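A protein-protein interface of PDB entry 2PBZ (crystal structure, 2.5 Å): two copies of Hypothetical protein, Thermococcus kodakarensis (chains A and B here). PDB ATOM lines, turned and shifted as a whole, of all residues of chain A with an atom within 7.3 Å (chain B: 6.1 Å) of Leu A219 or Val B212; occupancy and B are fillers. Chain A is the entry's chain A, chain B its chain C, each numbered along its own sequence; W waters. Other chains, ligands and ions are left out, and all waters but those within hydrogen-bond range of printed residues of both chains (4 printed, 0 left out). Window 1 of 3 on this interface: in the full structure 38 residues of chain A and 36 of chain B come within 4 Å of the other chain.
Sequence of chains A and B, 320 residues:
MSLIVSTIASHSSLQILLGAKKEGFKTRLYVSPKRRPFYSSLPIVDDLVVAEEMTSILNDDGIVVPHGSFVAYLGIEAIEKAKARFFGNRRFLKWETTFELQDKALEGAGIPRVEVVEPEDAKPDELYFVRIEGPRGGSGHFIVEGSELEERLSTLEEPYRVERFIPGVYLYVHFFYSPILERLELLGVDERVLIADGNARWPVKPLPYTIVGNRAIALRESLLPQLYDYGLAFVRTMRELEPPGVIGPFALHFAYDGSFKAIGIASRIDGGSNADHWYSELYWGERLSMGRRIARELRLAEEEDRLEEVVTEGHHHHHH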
ATOM      1  N   GLY A 168      31.023   7.087  -4.979  1.00  0.00           N
ATOM      2  CA  GLY A 168      29.845   6.974  -4.139  1.00  0.00           C
ATOM      3  C   GLY A 168      29.501   8.131  -3.238  1.00  0.00           C
ATOM      4  O   GLY A 168      29.867   8.147  -2.072  1.00  0.00           O
ATOM      5  N   VAL A 169      28.764   9.085  -3.787  1.00  0.00           N
ATOM      6  CA  VAL A 169      28.324  10.261  -3.068  1.00  0.00           C
ATOM      7  C   VAL A 169      29.225  10.778  -1.949  1.00  0.00           C
ATOM      8  O   VAL A 169      29.564  10.077  -0.976  1.00  0.00           O
ATOM      9  CB  VAL A 169      26.895  10.071  -2.500  1.00  0.00           C
ATOM     10  CG1 VAL A 169      26.880   9.007  -1.441  1.00  0.00           C
ATOM     11  CG2 VAL A 169      26.396  11.395  -1.943  1.00  0.00           C
ATOM     12  N   LEU A 171      29.528  13.451   0.939  1.00  0.00           N
ATOM     13  CA  LEU A 171      28.707  14.216   1.853  1.00  0.00           C
ATOM     14  C   LEU A 171      29.499  15.117   2.770  1.00  0.00           C
ATOM     15  O   LEU A 171      30.510  14.726   3.338  1.00  0.00           O
ATOM     16  CB  LEU A 171      27.871  13.240   2.672  1.00  0.00           C
ATOM     17  CG  LEU A 171      27.050  12.300   1.782  1.00  0.00           C
ATOM     18  CD1 LEU A 171      26.562  11.116   2.617  1.00  0.00           C
ATOM     19  CD2 LEU A 171      25.882  13.063   1.151  1.00  0.00           C
ATOM     20  N   VAL A 173      29.021  17.133   6.075  1.00  0.00           N
ATOM     21  CA  VAL A 173      28.196  17.357   7.247  1.00  0.00           C
ATOM     22  C   VAL A 173      28.589  18.606   8.000  1.00  0.00           C
ATOM     23  O   VAL A 173      29.738  18.791   8.364  1.00  0.00           O
ATOM     24  CB  VAL A 173      28.265  16.151   8.197  1.00  0.00           C
ATOM     25  CG1 VAL A 173      27.133  16.231   9.230  1.00  0.00           C
ATOM     26  CG2 VAL A 173      28.177  14.863   7.388  1.00  0.00           C
ATOM     27  N   LEU A 186      23.734  19.311  14.600  1.00  0.00           N
ATOM     28  CA  LEU A 186      23.952  18.762  13.255  1.00  0.00           C
ATOM     29  C   LEU A 186      22.958  19.584  12.434  1.00  0.00           C
ATOM     30  O   LEU A 186      21.755  19.331  12.469  1.00  0.00           O
ATOM     31  CB  LEU A 186      23.596  17.264  13.241  1.00  0.00           C
ATOM     32  CG  LEU A 186      23.707  16.317  12.031  1.00  0.00           C
ATOM     33  CD1 LEU A 186      24.239  17.042  10.828  1.00  0.00           C
ATOM     34  CD2 LEU A 186      24.590  15.129  12.394  1.00  0.00           C
ATOM     35  N   GLY A 188      23.085  20.347   8.853  1.00  0.00           N
ATOM     36  CA  GLY A 188      22.893  20.178   7.433  1.00  0.00           C
ATOM     37  C   GLY A 188      23.859  19.221   6.789  1.00  0.00           C
ATOM     38  O   GLY A 188      24.874  18.842   7.370  1.00  0.00           O
ATOM     39  N   VAL A 189      23.511  18.810   5.581  1.00  0.00           N
ATOM     40  CA  VAL A 189      24.359  17.928   4.808  1.00  0.00           C
ATOM     41  C   VAL A 189      24.358  18.483   3.395  1.00  0.00           C
ATOM     42  O   VAL A 189      23.325  18.635   2.753  1.00  0.00           O
ATOM     43  CB  VAL A 189      23.865  16.470   4.776  1.00  0.00           C
ATOM     44  CG1 VAL A 189      24.875  15.624   4.016  1.00  0.00           C
ATOM     45  CG2 VAL A 189      23.676  15.942   6.193  1.00  0.00           C
ATOM     46  N   ALA A 216      21.831  21.322  -1.280  1.00  0.00           N
ATOM     47  CA  ALA A 216      21.379  20.872   0.030  1.00  0.00           C
ATOM     48  C   ALA A 216      20.766  19.488  -0.188  1.00  0.00           C
ATOM     49  O   ALA A 216      20.001  19.281  -1.137  1.00  0.00           O
ATOM     50  CB  ALA A 216      20.332  21.826   0.600  1.00  0.00           C
ATOM     51  N   ILE A 217      21.108  18.537   0.677  1.00  0.00           N
ATOM     52  CA  ILE A 217      20.591  17.179   0.559  1.00  0.00           C
ATOM     53  C   ILE A 217      20.032  16.644   1.871  1.00  0.00           C
ATOM     54  O   ILE A 217      20.653  16.782   2.922  1.00  0.00           O
ATOM     55  CB  ILE A 217      21.700  16.211   0.029  1.00  0.00           C
ATOM     56  CG1 ILE A 217      21.395  14.773   0.441  1.00  0.00           C
ATOM     57  CG2 ILE A 217      23.056  16.611   0.562  1.00  0.00           C
ATOM     58  CD1 ILE A 217      22.444  13.784  -0.015  1.00  0.00           C
ATOM     59  N   ALA A 218      18.846  16.055   1.813  1.00  0.00           N
ATOM     60  CA  ALA A 218      18.236  15.475   3.002  1.00  0.00           C
ATOM     61  C   ALA A 218      18.736  14.036   3.114  1.00  0.00           C
ATOM     62  O   ALA A 218      18.284  13.138   2.402  1.00  0.00           O
ATOM     63  CB  ALA A 218      16.718  15.506   2.896  1.00  0.00           C
ATOM     64  N   LEU A 219      19.687  13.832   4.014  1.00  0.00           N
ATOM     65  CA  LEU A 219      20.283  12.527   4.237  1.00  0.00           C
ATOM     66  C   LEU A 219      19.296  11.504   4.796  1.00  0.00           C
ATOM     67  O   LEU A 219      18.374  11.857   5.543  1.00  0.00           O
ATOM     68  CB  LEU A 219      21.457  12.674   5.200  1.00  0.00           C
ATOM     69  CG  LEU A 219      22.421  11.493   5.234  1.00  0.00           C
ATOM     70  CD1 LEU A 219      23.262  11.503   3.971  1.00  0.00           C
ATOM     71  CD2 LEU A 219      23.297  11.579   6.460  1.00  0.00           C
ATOM     72  N   ARG A 220      19.483  10.235   4.432  1.00  0.00           N
ATOM     73  CA  ARG A 220      18.623   9.168   4.948  1.00  0.00           C
ATOM     74  C   ARG A 220      18.788   9.248   6.467  1.00  0.00           C
ATOM     75  O   ARG A 220      19.906   9.204   6.972  1.00  0.00           O
ATOM     76  CB  ARG A 220      19.087   7.807   4.428  1.00  0.00           C
ATOM     77  CG  ARG A 220      18.124   6.672   4.697  1.00  0.00           C
ATOM     78  CD  ARG A 220      18.879   5.423   5.131  1.00  0.00           C
ATOM     79  NE  ARG A 220      19.378   4.621   4.018  1.00  0.00           N
ATOM     80  CZ  ARG A 220      18.670   3.666   3.429  1.00  0.00           C
ATOM     81  NH1 ARG A 220      17.441   3.404   3.862  1.00  0.00           N
ATOM     82  NH2 ARG A 220      19.180   2.978   2.414  1.00  0.00           N
ATOM     83  N   GLU A 221      17.675   9.396   7.179  1.00  0.00           N
ATOM     84  CA  GLU A 221      17.675   9.533   8.631  1.00  0.00           C
ATOM     85  C   GLU A 221      18.424   8.472   9.447  1.00  0.00           C
ATOM     86  O   GLU A 221      18.934   8.770  10.532  1.00  0.00           O
ATOM     87  CB  GLU A 221      16.231   9.631   9.144  1.00  0.00           C
ATOM     88  CG  GLU A 221      16.137  10.047  10.596  1.00  0.00           C
ATOM     89  CD  GLU A 221      14.711  10.170  11.081  1.00  0.00           C
ATOM     90  OE1 GLU A 221      13.967  11.024  10.553  1.00  0.00           O
ATOM     91  OE2 GLU A 221      14.333   9.411  11.997  1.00  0.00           O
ATOM     92  N   SER A 222      18.497   7.247   8.942  1.00  0.00           N
ATOM     93  CA  SER A 222      19.183   6.180   9.671  1.00  0.00           C
ATOM     94  C   SER A 222      20.697   6.381   9.779  1.00  0.00           C
ATOM     95  O   SER A 222      21.355   5.678  10.540  1.00  0.00           O
ATOM     96  CB  SER A 222      18.909   4.821   9.012  1.00  0.00           C
ATOM     97  OG  SER A 222      19.658   4.677   7.806  1.00  0.00           O
ATOM     98  N   LEU A 223      21.241   7.330   9.024  1.00  0.00           N
ATOM     99  CA  LEU A 223      22.683   7.600   9.011  1.00  0.00           C
ATOM    100  C   LEU A 223      23.126   8.750   9.913  1.00  0.00           C
ATOM    101  O   LEU A 223      24.300   8.858  10.260  1.00  0.00           O
ATOM    102  CB  LEU A 223      23.132   7.940   7.592  1.00  0.00           C
ATOM    103  CG  LEU A 223      22.841   6.964   6.459  1.00  0.00           C
ATOM    104  CD1 LEU A 223      23.073   7.664   5.142  1.00  0.00           C
ATOM    105  CD2 LEU A 223      23.714   5.729   6.592  1.00  0.00           C
ATOM    106  N   LEU A 224      22.189   9.613  10.278  1.00  0.00           N
ATOM    107  CA  LEU A 224      22.497  10.766  11.101  1.00  0.00           C
ATOM    108  C   LEU A 224      23.083  10.461  12.470  1.00  0.00           C
ATOM    109  O   LEU A 224      24.055  11.099  12.878  1.00  0.00           O
ATOM    110  CB  LEU A 224      21.254  11.640  11.265  1.00  0.00           C
ATOM    111  CG  LEU A 224      20.752  12.273   9.979  1.00  0.00           C
ATOM    112  CD1 LEU A 224      19.537  13.123  10.284  1.00  0.00           C
ATOM    113  CD2 LEU A 224      21.863  13.097   9.349  1.00  0.00           C
ATOM    114  N   PRO A 225      22.500   9.501  13.210  1.00  0.00           N
ATOM    115  CA  PRO A 225      23.018   9.162  14.540  1.00  0.00           C
ATOM    116  C   PRO A 225      24.524   8.894  14.521  1.00  0.00           C
ATOM    117  O   PRO A 225      25.278   9.375  15.357  1.00  0.00           O
ATOM    118  CB  PRO A 225      22.214   7.919  14.904  1.00  0.00           C
ATOM    119  CG  PRO A 225      20.900   8.184  14.258  1.00  0.00           C
ATOM    120  CD  PRO A 225      21.304   8.696  12.898  1.00  0.00           C
ATOM    121  N   LEU A 227      26.739   9.942  12.417  1.00  0.00           N
ATOM    122  CA  LEU A 227      27.493  11.161  12.159  1.00  0.00           C
ATOM    123  C   LEU A 227      27.583  12.010  13.417  1.00  0.00           C
ATOM    124  O   LEU A 227      28.609  12.620  13.704  1.00  0.00           O
ATOM    125  CB  LEU A 227      26.837  11.945  11.018  1.00  0.00           C
ATOM    126  CG  LEU A 227      26.949  11.273   9.644  1.00  0.00           C
ATOM    127  CD1 LEU A 227      26.124  12.035   8.634  1.00  0.00           C
ATOM    128  CD2 LEU A 227      28.410  11.210   9.197  1.00  0.00           C
ATOM    129  N   TYR A 256      30.803   8.207   1.072  1.00  0.00           N
ATOM    130  CA  TYR A 256      29.927   7.122   1.483  1.00  0.00           C
ATOM    131  C   TYR A 256      30.031   5.938   0.518  1.00  0.00           C
ATOM    132  O   TYR A 256      29.580   5.998  -0.629  1.00  0.00           O
ATOM    133  CB  TYR A 256      28.482   7.597   1.601  1.00  0.00           C
ATOM    134  CG  TYR A 256      27.627   6.617   2.359  1.00  0.00           C
ATOM    135  CD1 TYR A 256      27.928   6.279   3.676  1.00  0.00           C
ATOM    136  CD2 TYR A 256      26.549   5.992   1.755  1.00  0.00           C
ATOM    137  CE1 TYR A 256      27.178   5.336   4.374  1.00  0.00           C
ATOM    138  CE2 TYR A 256      25.786   5.039   2.447  1.00  0.00           C
ATOM    139  CZ  TYR A 256      26.110   4.716   3.762  1.00  0.00           C
ATOM    140  OH  TYR A 256      25.376   3.774   4.452  1.00  0.00           O
ATOM    141  N   ASP A 257      30.656   4.875   1.020  1.00  0.00           N
ATOM    142  CA  ASP A 257      30.913   3.610   0.307  1.00  0.00           C
ATOM    143  C   ASP A 257      29.685   2.789   0.604  1.00  0.00           C
ATOM    144  O   ASP A 257      29.229   1.977  -0.179  1.00  0.00           O
ATOM    145  CB  ASP A 257      32.100   2.898   0.980  1.00  0.00           C
ATOM    146  CG  ASP A 257      33.167   2.458   0.011  1.00  0.00           C
ATOM    147  OD1 ASP A 257      34.126   1.796   0.476  1.00  0.00           O
ATOM    148  OD2 ASP A 257      33.062   2.774  -1.193  1.00  0.00           O
ATOM    149  N   GLY A 258      29.187   3.049   1.801  1.00  0.00           N
ATOM    150  CA  GLY A 258      28.056   2.353   2.361  1.00  0.00           C
ATOM    151  C   GLY A 258      28.613   2.097   3.741  1.00  0.00           C
ATOM    152  O   GLY A 258      28.056   1.322   4.513  1.00  0.00           O
ATOM    153  N   PHE A 260      30.992   4.990   5.359  1.00  0.00           N
ATOM    154  CA  PHE A 260      31.722   6.192   5.823  1.00  0.00           C
ATOM    155  C   PHE A 260      33.235   6.139   6.064  1.00  0.00           C
ATOM    156  O   PHE A 260      33.727   5.415   6.932  1.00  0.00           O
ATOM    157  CB  PHE A 260      31.092   6.742   7.117  1.00  0.00           C
ATOM    158  CG  PHE A 260      29.816   7.506   6.898  1.00  0.00           C
ATOM    159  CD1 PHE A 260      28.742   7.368   7.776  1.00  0.00           C
ATOM    160  CD2 PHE A 260      29.678   8.354   5.799  1.00  0.00           C
ATOM    161  CE1 PHE A 260      27.553   8.058   7.558  1.00  0.00           C
ATOM    162  CE2 PHE A 260      28.486   9.055   5.571  1.00  0.00           C
ATOM    163  CZ  PHE A 260      27.422   8.904   6.455  1.00  0.00           C
ATOM    164  N   TRP A 278      17.499  22.627   6.441  1.00  0.00           N
ATOM    165  CA  TRP A 278      16.521  22.849   7.503  1.00  0.00           C
ATOM    166  C   TRP A 278      17.244  22.258   8.728  1.00  0.00           C
ATOM    167  O   TRP A 278      18.289  22.793   9.098  1.00  0.00           O
ATOM    168  CB  TRP A 278      15.150  22.193   7.205  1.00  0.00           C
ATOM    169  CG  TRP A 278      15.137  20.731   6.888  1.00  0.00           C
ATOM    170  CD1 TRP A 278      15.556  20.141   5.736  1.00  0.00           C
ATOM    171  CD2 TRP A 278      14.669  19.672   7.735  1.00  0.00           C
ATOM    172  NE1 TRP A 278      15.377  18.782   5.807  1.00  0.00           N
ATOM    173  CE2 TRP A 278      14.836  18.463   7.024  1.00  0.00           C
ATOM    174  CE3 TRP A 278      14.129  19.625   9.030  1.00  0.00           C
ATOM    175  CZ2 TRP A 278      14.480  17.215   7.562  1.00  0.00           C
ATOM    176  CZ3 TRP A 278      13.776  18.381   9.567  1.00  0.00           C
ATOM    177  CH2 TRP A 278      13.954  17.196   8.832  1.00  0.00           C
ATOM    178  N   TYR A 279      16.771  21.186   9.352  1.00  0.00           N
ATOM    179  CA  TYR A 279      17.523  20.641  10.504  1.00  0.00           C
ATOM    180  C   TYR A 279      17.595  21.591  11.705  1.00  0.00           C
ATOM    181  O   TYR A 279      17.205  21.222  12.803  1.00  0.00           O
ATOM    182  CB  TYR A 279      18.952  20.263  10.096  1.00  0.00           C
ATOM    183  CG  TYR A 279      19.054  18.967   9.340  1.00  0.00           C
ATOM    184  CD1 TYR A 279      17.939  18.405   8.723  1.00  0.00           C
ATOM    185  CD2 TYR A 279      20.275  18.328   9.191  1.00  0.00           C
ATOM    186  CE1 TYR A 279      18.042  17.241   7.971  1.00  0.00           C
ATOM    187  CE2 TYR A 279      20.386  17.165   8.440  1.00  0.00           C
ATOM    188  CZ  TYR A 279      19.270  16.626   7.829  1.00  0.00           C
ATOM    189  OH  TYR A 279      19.385  15.499   7.060  1.00  0.00           O
ATOM    190  N   HIS B  11      14.078   6.581   9.570  1.00  0.00           N
ATOM    191  CA  HIS B  11      13.364   6.892   8.336  1.00  0.00           C
ATOM    192  C   HIS B  11      12.980   8.364   8.190  1.00  0.00           C
ATOM    193  O   HIS B  11      13.636   9.119   7.486  1.00  0.00           O
ATOM    194  CB  HIS B  11      12.105   6.023   8.212  1.00  0.00           C
ATOM    195  CG  HIS B  11      11.410   6.157   6.892  1.00  0.00           C
ATOM    196  ND1 HIS B  11      11.837   5.506   5.756  1.00  0.00           N
ATOM    197  CD2 HIS B  11      10.341   6.905   6.519  1.00  0.00           C
ATOM    198  CE1 HIS B  11      11.063   5.847   4.742  1.00  0.00           C
ATOM    199  NE2 HIS B  11      10.147   6.694   5.178  1.00  0.00           N
ATOM    200  N   VAL B 193      19.474  10.103  -3.841  1.00  0.00           N
ATOM    201  CA  VAL B 193      20.925  10.247  -3.912  1.00  0.00           C
ATOM    202  C   VAL B 193      21.397   8.824  -3.619  1.00  0.00           C
ATOM    203  O   VAL B 193      21.266   8.332  -2.495  1.00  0.00           O
ATOM    204  CB  VAL B 193      21.507  11.233  -2.861  1.00  0.00           C
ATOM    205  CG1 VAL B 193      23.044  11.309  -3.015  1.00  0.00           C
ATOM    206  CG2 VAL B 193      20.905  12.627  -3.054  1.00  0.00           C
ATOM    207  N   LEU B 194      21.893   8.157  -4.660  1.00  0.00           N
ATOM    208  CA  LEU B 194      22.366   6.783  -4.564  1.00  0.00           C
ATOM    209  C   LEU B 194      23.871   6.732  -4.494  1.00  0.00           C
ATOM    210  O   LEU B 194      24.529   7.722  -4.826  1.00  0.00           O
ATOM    211  CB  LEU B 194      21.882   5.973  -5.783  1.00  0.00           C
ATOM    212  CG  LEU B 194      20.483   5.365  -5.721  1.00  0.00           C
ATOM    213  CD1 LEU B 194      19.505   6.342  -5.132  1.00  0.00           C
ATOM    214  CD2 LEU B 194      20.056   4.953  -7.109  1.00  0.00           C
ATOM    215  N   ILE B 195      24.414   5.588  -4.078  1.00  0.00           N
ATOM    216  CA  ILE B 195      25.849   5.466  -3.983  1.00  0.00           C
ATOM    217  C   ILE B 195      26.315   5.222  -5.393  1.00  0.00           C
ATOM    218  O   ILE B 195      27.507   5.282  -5.696  1.00  0.00           O
ATOM    219  CB  ILE B 195      26.271   4.340  -2.987  1.00  0.00           C
ATOM    220  CG1 ILE B 195      26.209   2.958  -3.594  1.00  0.00           C
ATOM    221  CG2 ILE B 195      25.329   4.347  -1.821  1.00  0.00           C
ATOM    222  CD1 ILE B 195      26.330   1.867  -2.527  1.00  0.00           C
ATOM    223  N   THR B 210      21.586   1.644  -3.341  1.00  0.00           N
ATOM    224  CA  THR B 210      21.153   1.999  -1.990  1.00  0.00           C
ATOM    225  C   THR B 210      21.074   3.530  -1.828  1.00  0.00           C
ATOM    226  O   THR B 210      22.028   4.254  -2.171  1.00  0.00           O
ATOM    227  CB  THR B 210      22.154   1.453  -0.940  1.00  0.00           C
ATOM    228  OG1 THR B 210      22.461   0.087  -1.237  1.00  0.00           O
ATOM    229  CG2 THR B 210      21.572   1.573   0.467  1.00  0.00           C
ATOM    230  N   ILE B 211      19.956   4.028  -1.298  1.00  0.00           N
ATOM    231  CA  ILE B 211      19.827   5.468  -1.128  1.00  0.00           C
ATOM    232  C   ILE B 211      20.615   5.970   0.072  1.00  0.00           C
ATOM    233  O   ILE B 211      20.674   5.315   1.132  1.00  0.00           O
ATOM    234  CB  ILE B 211      18.356   5.917  -0.956  1.00  0.00           C
ATOM    235  CG1 ILE B 211      17.949   5.793   0.510  1.00  0.00           C
ATOM    236  CG2 ILE B 211      17.418   5.068  -1.850  1.00  0.00           C
ATOM    237  CD1 ILE B 211      17.284   7.039   1.057  1.00  0.00           C
ATOM    238  N   VAL B 212      21.219   7.142  -0.102  1.00  0.00           N
ATOM    239  CA  VAL B 212      21.989   7.759   0.948  1.00  0.00           C
ATOM    240  C   VAL B 212      21.198   8.970   1.429  1.00  0.00           C
ATOM    241  O   VAL B 212      21.229   9.333   2.613  1.00  0.00           O
ATOM    242  CB  VAL B 212      23.346   8.217   0.406  1.00  0.00           C
ATOM    243  CG1 VAL B 212      24.302   8.522   1.567  1.00  0.00           C
ATOM    244  CG2 VAL B 212      23.911   7.146  -0.509  1.00  0.00           C
ATOM    245  N   GLY B 213      20.477   9.588   0.496  1.00  0.00           N
ATOM    246  CA  GLY B 213      19.687  10.768   0.810  1.00  0.00           C
ATOM    247  C   GLY B 213      18.677  11.125  -0.263  1.00  0.00           C
ATOM    248  O   GLY B 213      18.402  10.342  -1.154  1.00  0.00           O
ATOM    249  N   ASN B 214      18.139  12.334  -0.181  1.00  0.00           N
ATOM    250  CA  ASN B 214      17.129  12.781  -1.126  1.00  0.00           C
ATOM    251  C   ASN B 214      17.323  14.245  -1.515  1.00  0.00           C
ATOM    252  O   ASN B 214      17.697  15.065  -0.678  1.00  0.00           O
ATOM    253  CB  ASN B 214      15.745  12.605  -0.488  1.00  0.00           C
ATOM    254  CG  ASN B 214      15.498  11.176   0.009  1.00  0.00           C
ATOM    255  OD1 ASN B 214      15.035  10.322  -0.745  1.00  0.00           O
ATOM    256  ND2 ASN B 214      15.806  10.919   1.274  1.00  0.00           N
ATOM    257  N   ASN B 274      11.630  14.164   3.185  1.00  0.00           N
ATOM    258  CA  ASN B 274      12.504  14.836   4.153  1.00  0.00           C
ATOM    259  C   ASN B 274      13.160  16.026   3.436  1.00  0.00           C
ATOM    260  O   ASN B 274      13.652  16.949   4.086  1.00  0.00           O
ATOM    261  CB  ASN B 274      13.629  13.923   4.680  1.00  0.00           C
ATOM    262  CG  ASN B 274      13.139  12.859   5.652  1.00  0.00           C
ATOM    263  OD1 ASN B 274      12.318  13.125   6.530  1.00  0.00           O
ATOM    264  ND2 ASN B 274      13.667  11.655   5.515  1.00  0.00           N
HETATM  265  O   HOH W   1      15.877  11.767   3.887  1.00  0.00           O
HETATM  266  O   HOH W   2      15.273   8.226   4.994  1.00  0.00           O
HETATM  267  O   HOH W   3      13.817  13.296   8.771  1.00  0.00           O
HETATM  268  O   HOH W   4      16.219   5.887   7.575  1.00  0.00           O
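The backbone carbonyl oxygen of Ile B211 lies within hydrogen-bond range of the guanidinium group of Arg A220, 3.1 Å away.
O of Val B212 sits at hydrogen-bond distance from N of Arg A220 (2.7 Å).
The backbone NH (N) of Asn B214 lies within hydrogen-bond range of the backbone carbonyl oxygen (O) of Ala A218 (2.7 Å).
The indole nitrogen of Trp A278 sits at hydrogen-bond distance from the backbone carbonyl oxygen of Asn B274 (3.0 Å).
Water W3 bridges the side-chain amide oxygen (OD1) of Asn B274 (2.7 Å) and the side-chain carboxylate (OE1) of Glu A221 (2.9 Å).
Water W1 lies within hydrogen-bond range of the side-chain amide nitrogen (ND2) of Asn B274, the side-chain amide nitrogen (ND2) of Asn B214, the backbone carbonyl oxygen (O) of Leu A219 and the backbone carbonyl oxygen (O) of Ala A218.
Water W4 bridges N of Ser A222 and N of His B11.
Water W2 bridges the backbone carbonyl oxygen (O) of His B11 (3.1 Å) and the backbone NH (N) of Glu A221 (3.5 Å).
Leu A219 touches just these residues of chain B: Val B212 and Gly B213.
Val B212 touches just these residues of chain A: Val A169, Leu A171, Leu A219, Arg A220, Leu A223 and Tyr A256.
Of the printed residues of chain A, His B11 touches Glu A221.
Of the printed residues of chain A, Ile B195 touches Gly A168 and Asp A257.
Of the printed residues of chain A, Gly B213 touches Ala A218, Leu A219 and Arg A220.
Printed residues of chain A within 4 Å of Asn B274: Ala A218 and Trp A278.
The backbone NH (N) of Val B212 sits at hydrogen-bond distance from the backbone carbonyl oxygen (O) of Val B193, at 2.7 Å.
O of Gly B213 is in hydrogen-bond range of N of Val B193 (2.9 Å).
N of Tyr A256 lies within hydrogen-bond range of O of Gly A168.
OH of Tyr A279 is in hydrogen-bond range of N of Leu A219, 3.5 Å away.
The backbone NH of Ile A217 lies close to the backbone carbonyl oxygen of Val A189, 3.0 Å away.
The side-chain amide nitrogen (ND2) of Asn B274 lies within hydrogen-bond range of the backbone carbonyl oxygen (O) of His B11 (3.2 Å).
No position is printed for both chains.
Of the 20 pairs that touch across the chains among the printed residues, none has its exchanged pair printed and touching as well.
Of the 24 printed residues of chain A, 12 touch a printed residue of chain B.
Hydrophobic or aromatic side chains of chain A within 4 Å of the printed part of chain B: Val A169, Leu A171, Ile A217, Ala A218, Leu A219, Leu A223, Tyr A256 and Trp A278.
Printed residues of chain B that touch a printed residue of chain A: His B11, Val B193, Ile B195, Thr B210, Ile B211, Val B212, Gly B213, Asn B214 and Asn B274.
Hydrophobic or aromatic side chains of chain B that line the printed part of chain A: Val B193, Ile B195, Ile B211 and Val B212.
Among the printed residues, 20 pairs touch across the chains.
Among the printed residues, merely in contact across the chains: Gly A168 with Ile B195 (3.3 Å), Val A169 with Val B193 (3.5 Å), Val A169 with Val B212 (3.6 Å), Leu A171 with Val B212 (3.6 Å), Ile A217 with Val B193 (3.6 Å), Ile A217 with Asn B214 (3.8 Å), Ala A218 with Gly B213 (3.2 Å), Ala A218 with Asn B274 (3.6 Å), Leu A219 with Val B212 (3.3 Å), Leu A219 with Gly B213 (3.9 Å), Arg A220 with Thr B210 (3.4 Å), Arg A220 with Gly B213 (3.7 Å), Glu A221 with His B11 (3.1 Å), Leu A223 with Val B212 (3.5 Å), Tyr A256 with Val B212 (3.4 Å) and Asp A257 with Ile B195 (3.7 Å).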
